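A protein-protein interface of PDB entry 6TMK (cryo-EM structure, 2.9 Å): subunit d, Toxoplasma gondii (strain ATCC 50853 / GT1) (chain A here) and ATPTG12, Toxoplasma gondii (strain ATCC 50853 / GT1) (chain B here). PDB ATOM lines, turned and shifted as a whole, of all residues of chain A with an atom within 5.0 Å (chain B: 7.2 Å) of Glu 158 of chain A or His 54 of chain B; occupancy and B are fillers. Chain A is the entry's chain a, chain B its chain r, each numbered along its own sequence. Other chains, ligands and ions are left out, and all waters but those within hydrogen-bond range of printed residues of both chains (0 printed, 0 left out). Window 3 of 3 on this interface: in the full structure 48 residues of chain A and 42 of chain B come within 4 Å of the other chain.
The backbone NH (N) of His 54 of chain B sits at hydrogen-bond distance from the side-chain carboxylate (OE1) of Glu 158 of chain A (3.3 Å). OH of Tyr 53 of chain B is in hydrogen-bond range of OD2 of Asp 161 of chain A, at 3.0 Å.
The backbone carbonyl oxygen (O) of Trp 159 of chain A is in hydrogen-bond range of the side-chain hydroxyl (OG) of Ser 162 of chain A (2.7 Å). The backbone NH of Tyr 53 of chain B is in hydrogen-bond range of the backbone carbonyl oxygen of Tyr 58 of chain B (2.7 Å).
Pro 149 of chain A touches Tyr 58 of chain B (CG to CZ, 3.7 Å). Phe 4 of chain B touches Val 154 of chain A. Tyr 53 of chain B touches Glu 158 of chain A (CD1 to CG, 3.7 Å). O of Ser 162 of chain A touches ND2 of Asn 3 of chain B, 3.98 Å away. OG of Ser 162 of chain A touches CE2 of Phe 4 of chain B, at 3.8 Å. Tyr 53 of chain B touches Ser 162 of chain A.
Of the printed residues of chain B, Glu 158 of chain A touches Tyr 53 and His 54. His 54 of chain B touches one residue of chain A. Printed residues of chain A within 4 Å of Asn 3 of chain B: Ser 162. Of the printed residues of chain B, Ser 162 of chain A touches Asn 3, Phe 4 and Tyr 53. Printed residues of chain B within 4 Å of Pro 149 of chain A: Tyr 58 (3.7 Å). Printed residues of chain B within 4 Å of Asp 161 of chain A: Tyr 53 (3.0 Å). Of the printed residues of chain A, Tyr 58 of chain B touches Pro 149 (3.7 Å). The nearest residue of chain B that does not touch Glu 158 of chain A is Phe 4 of chain B (4.1 Å).
Of the 11 printed residues of chain A, 5 touch a printed residue of chain B. Hydrophobic or aromatic side chains of chain A that line the printed part of chain B: Pro 149 and Val 154. Along chain A the printed residues that touch a printed residue of chain B span positions 149 to 162. Hydrophobic or aromatic side chains of chain B within 4 Å of the printed part of chain A: Phe 4, Tyr 53 and Tyr 58. Among the printed residues, 8 pairs touch across the chains. Among the printed residues, no Asp or Glu carboxylate lies within 4 Å of a Lys or Arg side-chain nitrogen of the other chain.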
ATOM      1  N   PRO A 149       8.149  25.326   7.552  1.00  0.00           N
ATOM      2  CA  PRO A 149       8.454  24.011   7.016  1.00  0.00           C
ATOM      3  C   PRO A 149       9.866  23.967   6.465  1.00  0.00           C
ATOM      4  O   PRO A 149      10.518  25.011   6.322  1.00  0.00           O
ATOM      5  CB  PRO A 149       7.414  23.831   5.899  1.00  0.00           C
ATOM      6  CG  PRO A 149       6.468  24.953   6.037  1.00  0.00           C
ATOM      7  CD  PRO A 149       7.214  26.048   6.679  1.00  0.00           C
ATOM      8  N   LYS A 153      11.177  21.134   1.126  1.00  0.00           N
ATOM      9  CA  LYS A 153       9.835  20.592   0.987  1.00  0.00           C
ATOM     10  C   LYS A 153       8.876  21.622   0.416  1.00  0.00           C
ATOM     11  O   LYS A 153       7.894  21.257  -0.235  1.00  0.00           O
ATOM     12  CB  LYS A 153       9.320  20.115   2.340  1.00  0.00           C
ATOM     13  CG  LYS A 153       9.794  18.754   2.750  1.00  0.00           C
ATOM     14  CD  LYS A 153       9.315  18.429   4.141  1.00  0.00           C
ATOM     15  CE  LYS A 153       9.413  16.959   4.446  1.00  0.00           C
ATOM     16  NZ  LYS A 153      10.810  16.506   4.464  1.00  0.00           N
ATOM     17  N   VAL A 154       9.135  22.901   0.667  1.00  0.00           N
ATOM     18  CA  VAL A 154       8.226  23.947   0.221  1.00  0.00           C
ATOM     19  C   VAL A 154       8.247  24.049  -1.299  1.00  0.00           C
ATOM     20  O   VAL A 154       9.292  23.885  -1.941  1.00  0.00           O
ATOM     21  CB  VAL A 154       8.592  25.287   0.873  1.00  0.00           C
ATOM     22  CG1 VAL A 154       7.824  26.401   0.228  1.00  0.00           C
ATOM     23  CG2 VAL A 154       8.297  25.230   2.341  1.00  0.00           C
ATOM     24  N   ASN A 155       7.081  24.323  -1.880  1.00  0.00           N
ATOM     25  CA  ASN A 155       6.976  24.546  -3.314  1.00  0.00           C
ATOM     26  C   ASN A 155       7.665  25.849  -3.696  1.00  0.00           C
ATOM     27  O   ASN A 155       7.576  26.853  -2.986  1.00  0.00           O
ATOM     28  CB  ASN A 155       5.504  24.580  -3.725  1.00  0.00           C
ATOM     29  CG  ASN A 155       5.300  24.554  -5.221  1.00  0.00           C
ATOM     30  OD1 ASN A 155       4.741  25.484  -5.796  1.00  0.00           O
ATOM     31  ND2 ASN A 155       5.721  23.474  -5.853  1.00  0.00           N
ATOM     32  N   THR A 156       8.346  25.830  -4.839  1.00  0.00           N
ATOM     33  CA  THR A 156       9.168  26.962  -5.253  1.00  0.00           C
ATOM     34  C   THR A 156       8.317  28.186  -5.575  1.00  0.00           C
ATOM     35  O   THR A 156       8.618  29.303  -5.131  1.00  0.00           O
ATOM     36  CB  THR A 156      10.019  26.550  -6.450  1.00  0.00           C
ATOM     37  OG1 THR A 156      10.591  25.264  -6.202  1.00  0.00           O
ATOM     38  CG2 THR A 156      11.127  27.520  -6.682  1.00  0.00           C
ATOM     39  N   ASN A 157       7.252  28.000  -6.353  1.00  0.00           N
ATOM     40  CA  ASN A 157       6.413  29.129  -6.722  1.00  0.00           C
ATOM     41  C   ASN A 157       5.688  29.700  -5.515  1.00  0.00           C
ATOM     42  O   ASN A 157       5.451  30.909  -5.453  1.00  0.00           O
ATOM     43  CB  ASN A 157       5.418  28.703  -7.797  1.00  0.00           C
ATOM     44  CG  ASN A 157       5.071  29.820  -8.749  1.00  0.00           C
ATOM     45  OD1 ASN A 157       5.858  30.736  -8.974  1.00  0.00           O
ATOM     46  ND2 ASN A 157       3.884  29.747  -9.314  1.00  0.00           N
ATOM     47  N   GLU A 158       5.350  28.861  -4.538  1.00  0.00           N
ATOM     48  CA  GLU A 158       4.742  29.368  -3.316  1.00  0.00           C
ATOM     49  C   GLU A 158       5.723  30.224  -2.527  1.00  0.00           C
ATOM     50  O   GLU A 158       5.356  31.284  -2.006  1.00  0.00           O
ATOM     51  CB  GLU A 158       4.240  28.205  -2.467  1.00  0.00           C
ATOM     52  CG  GLU A 158       2.949  27.596  -2.955  1.00  0.00           C
ATOM     53  CD  GLU A 158       2.504  26.427  -2.107  1.00  0.00           C
ATOM     54  OE1 GLU A 158       3.315  25.944  -1.292  1.00  0.00           O
ATOM     55  OE2 GLU A 158       1.342  25.994  -2.252  1.00  0.00           O
ATOM     56  N   TRP A 159       6.974  29.779  -2.424  1.00  0.00           N
ATOM     57  CA  TRP A 159       7.990  30.597  -1.780  1.00  0.00           C
ATOM     58  C   TRP A 159       8.146  31.939  -2.476  1.00  0.00           C
ATOM     59  O   TRP A 159       8.246  32.982  -1.820  1.00  0.00           O
ATOM     60  CB  TRP A 159       9.325  29.857  -1.749  1.00  0.00           C
ATOM     61  CG  TRP A 159      10.436  30.725  -1.305  1.00  0.00           C
ATOM     62  CD1 TRP A 159      10.643  31.194  -0.052  1.00  0.00           C
ATOM     63  CD2 TRP A 159      11.498  31.244  -2.109  1.00  0.00           C
ATOM     64  NE1 TRP A 159      11.764  31.976  -0.018  1.00  0.00           N
ATOM     65  CE2 TRP A 159      12.310  32.022  -1.272  1.00  0.00           C
ATOM     66  CE3 TRP A 159      11.841  31.126  -3.454  1.00  0.00           C
ATOM     67  CZ2 TRP A 159      13.439  32.675  -1.733  1.00  0.00           C
ATOM     68  CZ3 TRP A 159      12.958  31.774  -3.905  1.00  0.00           C
ATOM     69  CH2 TRP A 159      13.746  32.537  -3.050  1.00  0.00           C
ATOM     70  N   LEU A 160       8.176  31.935  -3.807  1.00  0.00           N
ATOM     71  CA  LEU A 160       8.361  33.185  -4.527  1.00  0.00           C
ATOM     72  C   LEU A 160       7.133  34.080  -4.437  1.00  0.00           C
ATOM     73  O   LEU A 160       7.257  35.306  -4.519  1.00  0.00           O
ATOM     74  CB  LEU A 160       8.724  32.904  -5.975  1.00  0.00           C
ATOM     75  CG  LEU A 160       9.503  34.036  -6.629  1.00  0.00           C
ATOM     76  CD1 LEU A 160      10.944  34.004  -6.204  1.00  0.00           C
ATOM     77  CD2 LEU A 160       9.396  33.923  -8.110  1.00  0.00           C
ATOM     78  N   ASP A 161       5.947  33.496  -4.284  1.00  0.00           N
ATOM     79  CA  ASP A 161       4.757  34.303  -4.061  1.00  0.00           C
ATOM     80  C   ASP A 161       4.792  34.940  -2.683  1.00  0.00           C
ATOM     81  O   ASP A 161       4.366  36.087  -2.512  1.00  0.00           O
ATOM     82  CB  ASP A 161       3.505  33.448  -4.226  1.00  0.00           C
ATOM     83  CG  ASP A 161       2.243  34.275  -4.334  1.00  0.00           C
ATOM     84  OD1 ASP A 161       2.340  35.518  -4.298  1.00  0.00           O
ATOM     85  OD2 ASP A 161       1.151  33.683  -4.451  1.00  0.00           O
ATOM     86  N   SER A 162       5.293  34.211  -1.690  1.00  0.00           N
ATOM     87  CA  SER A 162       5.456  34.795  -0.366  1.00  0.00           C
ATOM     88  C   SER A 162       6.463  35.937  -0.395  1.00  0.00           C
ATOM     89  O   SER A 162       6.229  36.997   0.195  1.00  0.00           O
ATOM     90  CB  SER A 162       5.893  33.722   0.625  1.00  0.00           C
ATOM     91  OG  SER A 162       7.295  33.556   0.619  1.00  0.00           O
ATOM     92  N   ASN B   3       8.126  33.491   5.054  1.00  0.00           N
ATOM     93  CA  ASN B   3       6.858  34.152   5.354  1.00  0.00           C
ATOM     94  C   ASN B   3       5.702  33.155   5.283  1.00  0.00           C
ATOM     95  O   ASN B   3       4.787  33.255   4.469  1.00  0.00           O
ATOM     96  CB  ASN B   3       6.648  35.319   4.402  1.00  0.00           C
ATOM     97  CG  ASN B   3       5.538  36.229   4.834  1.00  0.00           C
ATOM     98  OD1 ASN B   3       4.894  36.004   5.855  1.00  0.00           O
ATOM     99  ND2 ASN B   3       5.300  37.268   4.055  1.00  0.00           N
ATOM    100  N   PHE B   4       5.773  32.172   6.176  1.00  0.00           N
ATOM    101  CA  PHE B   4       4.789  31.096   6.279  1.00  0.00           C
ATOM    102  C   PHE B   4       4.346  31.001   7.736  1.00  0.00           C
ATOM    103  O   PHE B   4       5.029  30.378   8.553  1.00  0.00           O
ATOM    104  CB  PHE B   4       5.377  29.771   5.811  1.00  0.00           C
ATOM    105  CG  PHE B   4       5.479  29.632   4.326  1.00  0.00           C
ATOM    106  CD1 PHE B   4       4.698  28.719   3.649  1.00  0.00           C
ATOM    107  CD2 PHE B   4       6.366  30.399   3.609  1.00  0.00           C
ATOM    108  CE1 PHE B   4       4.799  28.583   2.289  1.00  0.00           C
ATOM    109  CE2 PHE B   4       6.467  30.266   2.245  1.00  0.00           C
ATOM    110  CZ  PHE B   4       5.683  29.361   1.587  1.00  0.00           C
ATOM    111  N   GLU B  52      -2.635  31.797   1.068  1.00  0.00           N
ATOM    112  CA  GLU B  52      -2.572  30.554   1.817  1.00  0.00           C
ATOM    113  C   GLU B  52      -1.767  29.546   1.018  1.00  0.00           C
ATOM    114  O   GLU B  52      -2.038  29.331  -0.165  1.00  0.00           O
ATOM    115  CB  GLU B  52      -3.971  30.014   2.110  1.00  0.00           C
ATOM    116  CG  GLU B  52      -4.943  30.167   0.970  1.00  0.00           C
ATOM    117  CD  GLU B  52      -6.280  29.514   1.256  1.00  0.00           C
ATOM    118  OE1 GLU B  52      -6.486  29.057   2.400  1.00  0.00           O
ATOM    119  OE2 GLU B  52      -7.124  29.456   0.336  1.00  0.00           O
ATOM    120  N   TYR B  53      -0.778  28.942   1.666  1.00  0.00           N
ATOM    121  CA  TYR B  53       0.192  28.092   1.002  1.00  0.00           C
ATOM    122  C   TYR B  53       0.369  26.799   1.782  1.00  0.00           C
ATOM    123  O   TYR B  53      -0.059  26.672   2.930  1.00  0.00           O
ATOM    124  CB  TYR B  53       1.546  28.795   0.864  1.00  0.00           C
ATOM    125  CG  TYR B  53       1.496  30.165   0.242  1.00  0.00           C
ATOM    126  CD1 TYR B  53       1.186  30.331  -1.096  1.00  0.00           C
ATOM    127  CD2 TYR B  53       1.776  31.293   0.990  1.00  0.00           C
ATOM    128  CE1 TYR B  53       1.146  31.577  -1.665  1.00  0.00           C
ATOM    129  CE2 TYR B  53       1.739  32.544   0.426  1.00  0.00           C
ATOM    130  CZ  TYR B  53       1.424  32.682  -0.899  1.00  0.00           C
ATOM    131  OH  TYR B  53       1.386  33.936  -1.458  1.00  0.00           O
ATOM    132  N   HIS B  54       1.023  25.836   1.134  1.00  0.00           N
ATOM    133  CA  HIS B  54       1.448  24.586   1.757  1.00  0.00           C
ATOM    134  C   HIS B  54       0.250  23.821   2.331  1.00  0.00           C
ATOM    135  O   HIS B  54       0.106  23.628   3.537  1.00  0.00           O
ATOM    136  CB  HIS B  54       2.508  24.870   2.822  1.00  0.00           C
ATOM    137  CG  HIS B  54       3.389  23.702   3.127  1.00  0.00           C
ATOM    138  ND1 HIS B  54       3.286  22.973   4.291  1.00  0.00           N
ATOM    139  CD2 HIS B  54       4.397  23.143   2.420  1.00  0.00           C
ATOM    140  CE1 HIS B  54       4.193  22.013   4.285  1.00  0.00           C
ATOM    141  NE2 HIS B  54       4.877  22.093   3.160  1.00  0.00           N
ATOM    142  N   ASN B  55      -0.607  23.385   1.411  1.00  0.00           N
ATOM    143  CA  ASN B  55      -1.859  22.701   1.716  1.00  0.00           C
ATOM    144  C   ASN B  55      -2.878  23.612   2.378  1.00  0.00           C
ATOM    145  O   ASN B  55      -3.783  23.135   3.067  1.00  0.00           O
ATOM    146  CB  ASN B  55      -1.605  21.479   2.601  1.00  0.00           C
ATOM    147  CG  ASN B  55      -2.660  20.415   2.448  1.00  0.00           C
ATOM    148  OD1 ASN B  55      -3.098  20.107   1.343  1.00  0.00           O
ATOM    149  ND2 ASN B  55      -3.068  19.836   3.565  1.00  0.00           N
ATOM    150  N   LYS B  56      -2.750  24.919   2.176  1.00  0.00           N
ATOM    151  CA  LYS B  56      -3.629  25.902   2.800  1.00  0.00           C
ATOM    152  C   LYS B  56      -3.611  25.755   4.315  1.00  0.00           C
ATOM    153  O   LYS B  56      -4.647  25.791   4.981  1.00  0.00           O
ATOM    154  CB  LYS B  56      -5.045  25.799   2.242  1.00  0.00           C
ATOM    155  CG  LYS B  56      -5.110  26.125   0.767  1.00  0.00           C
ATOM    156  CD  LYS B  56      -6.516  26.039   0.225  1.00  0.00           C
ATOM    157  CE  LYS B  56      -6.509  25.870  -1.283  1.00  0.00           C
ATOM    158  NZ  LYS B  56      -5.397  26.629  -1.926  1.00  0.00           N
ATOM    159  N   ASP B  57      -2.410  25.583   4.855  1.00  0.00           N
ATOM    160  CA  ASP B  57      -2.170  25.520   6.283  1.00  0.00           C
ATOM    161  C   ASP B  57      -1.329  26.678   6.787  1.00  0.00           C
ATOM    162  O   ASP B  57      -1.205  26.853   8.004  1.00  0.00           O
ATOM    163  CB  ASP B  57      -1.478  24.202   6.639  1.00  0.00           C
ATOM    164  CG  ASP B  57      -2.355  22.996   6.384  1.00  0.00           C
ATOM    165  OD1 ASP B  57      -1.807  21.884   6.245  1.00  0.00           O
ATOM    166  OD2 ASP B  57      -3.590  23.156   6.325  1.00  0.00           O
ATOM    167  N   TYR B  58      -0.762  27.475   5.889  1.00  0.00           N
ATOM    168  CA  TYR B  58       0.075  28.607   6.241  1.00  0.00           C
ATOM    169  C   TYR B  58      -0.391  29.835   5.483  1.00  0.00           C
ATOM    170  O   TYR B  58      -0.600  29.781   4.269  1.00  0.00           O
ATOM    171  CB  TYR B  58       1.541  28.343   5.908  1.00  0.00           C
ATOM    172  CG  TYR B  58       2.208  27.261   6.713  1.00  0.00           C
ATOM    173  CD1 TYR B  58       3.086  27.574   7.730  1.00  0.00           C
ATOM    174  CD2 TYR B  58       1.982  25.927   6.440  1.00  0.00           C
ATOM    175  CE1 TYR B  58       3.706  26.601   8.457  1.00  0.00           C
ATOM    176  CE2 TYR B  58       2.597  24.941   7.166  1.00  0.00           C
ATOM    177  CZ  TYR B  58       3.461  25.283   8.175  1.00  0.00           C
ATOM    178  OH  TYR B  58       4.083  24.303   8.908  1.00  0.00           O
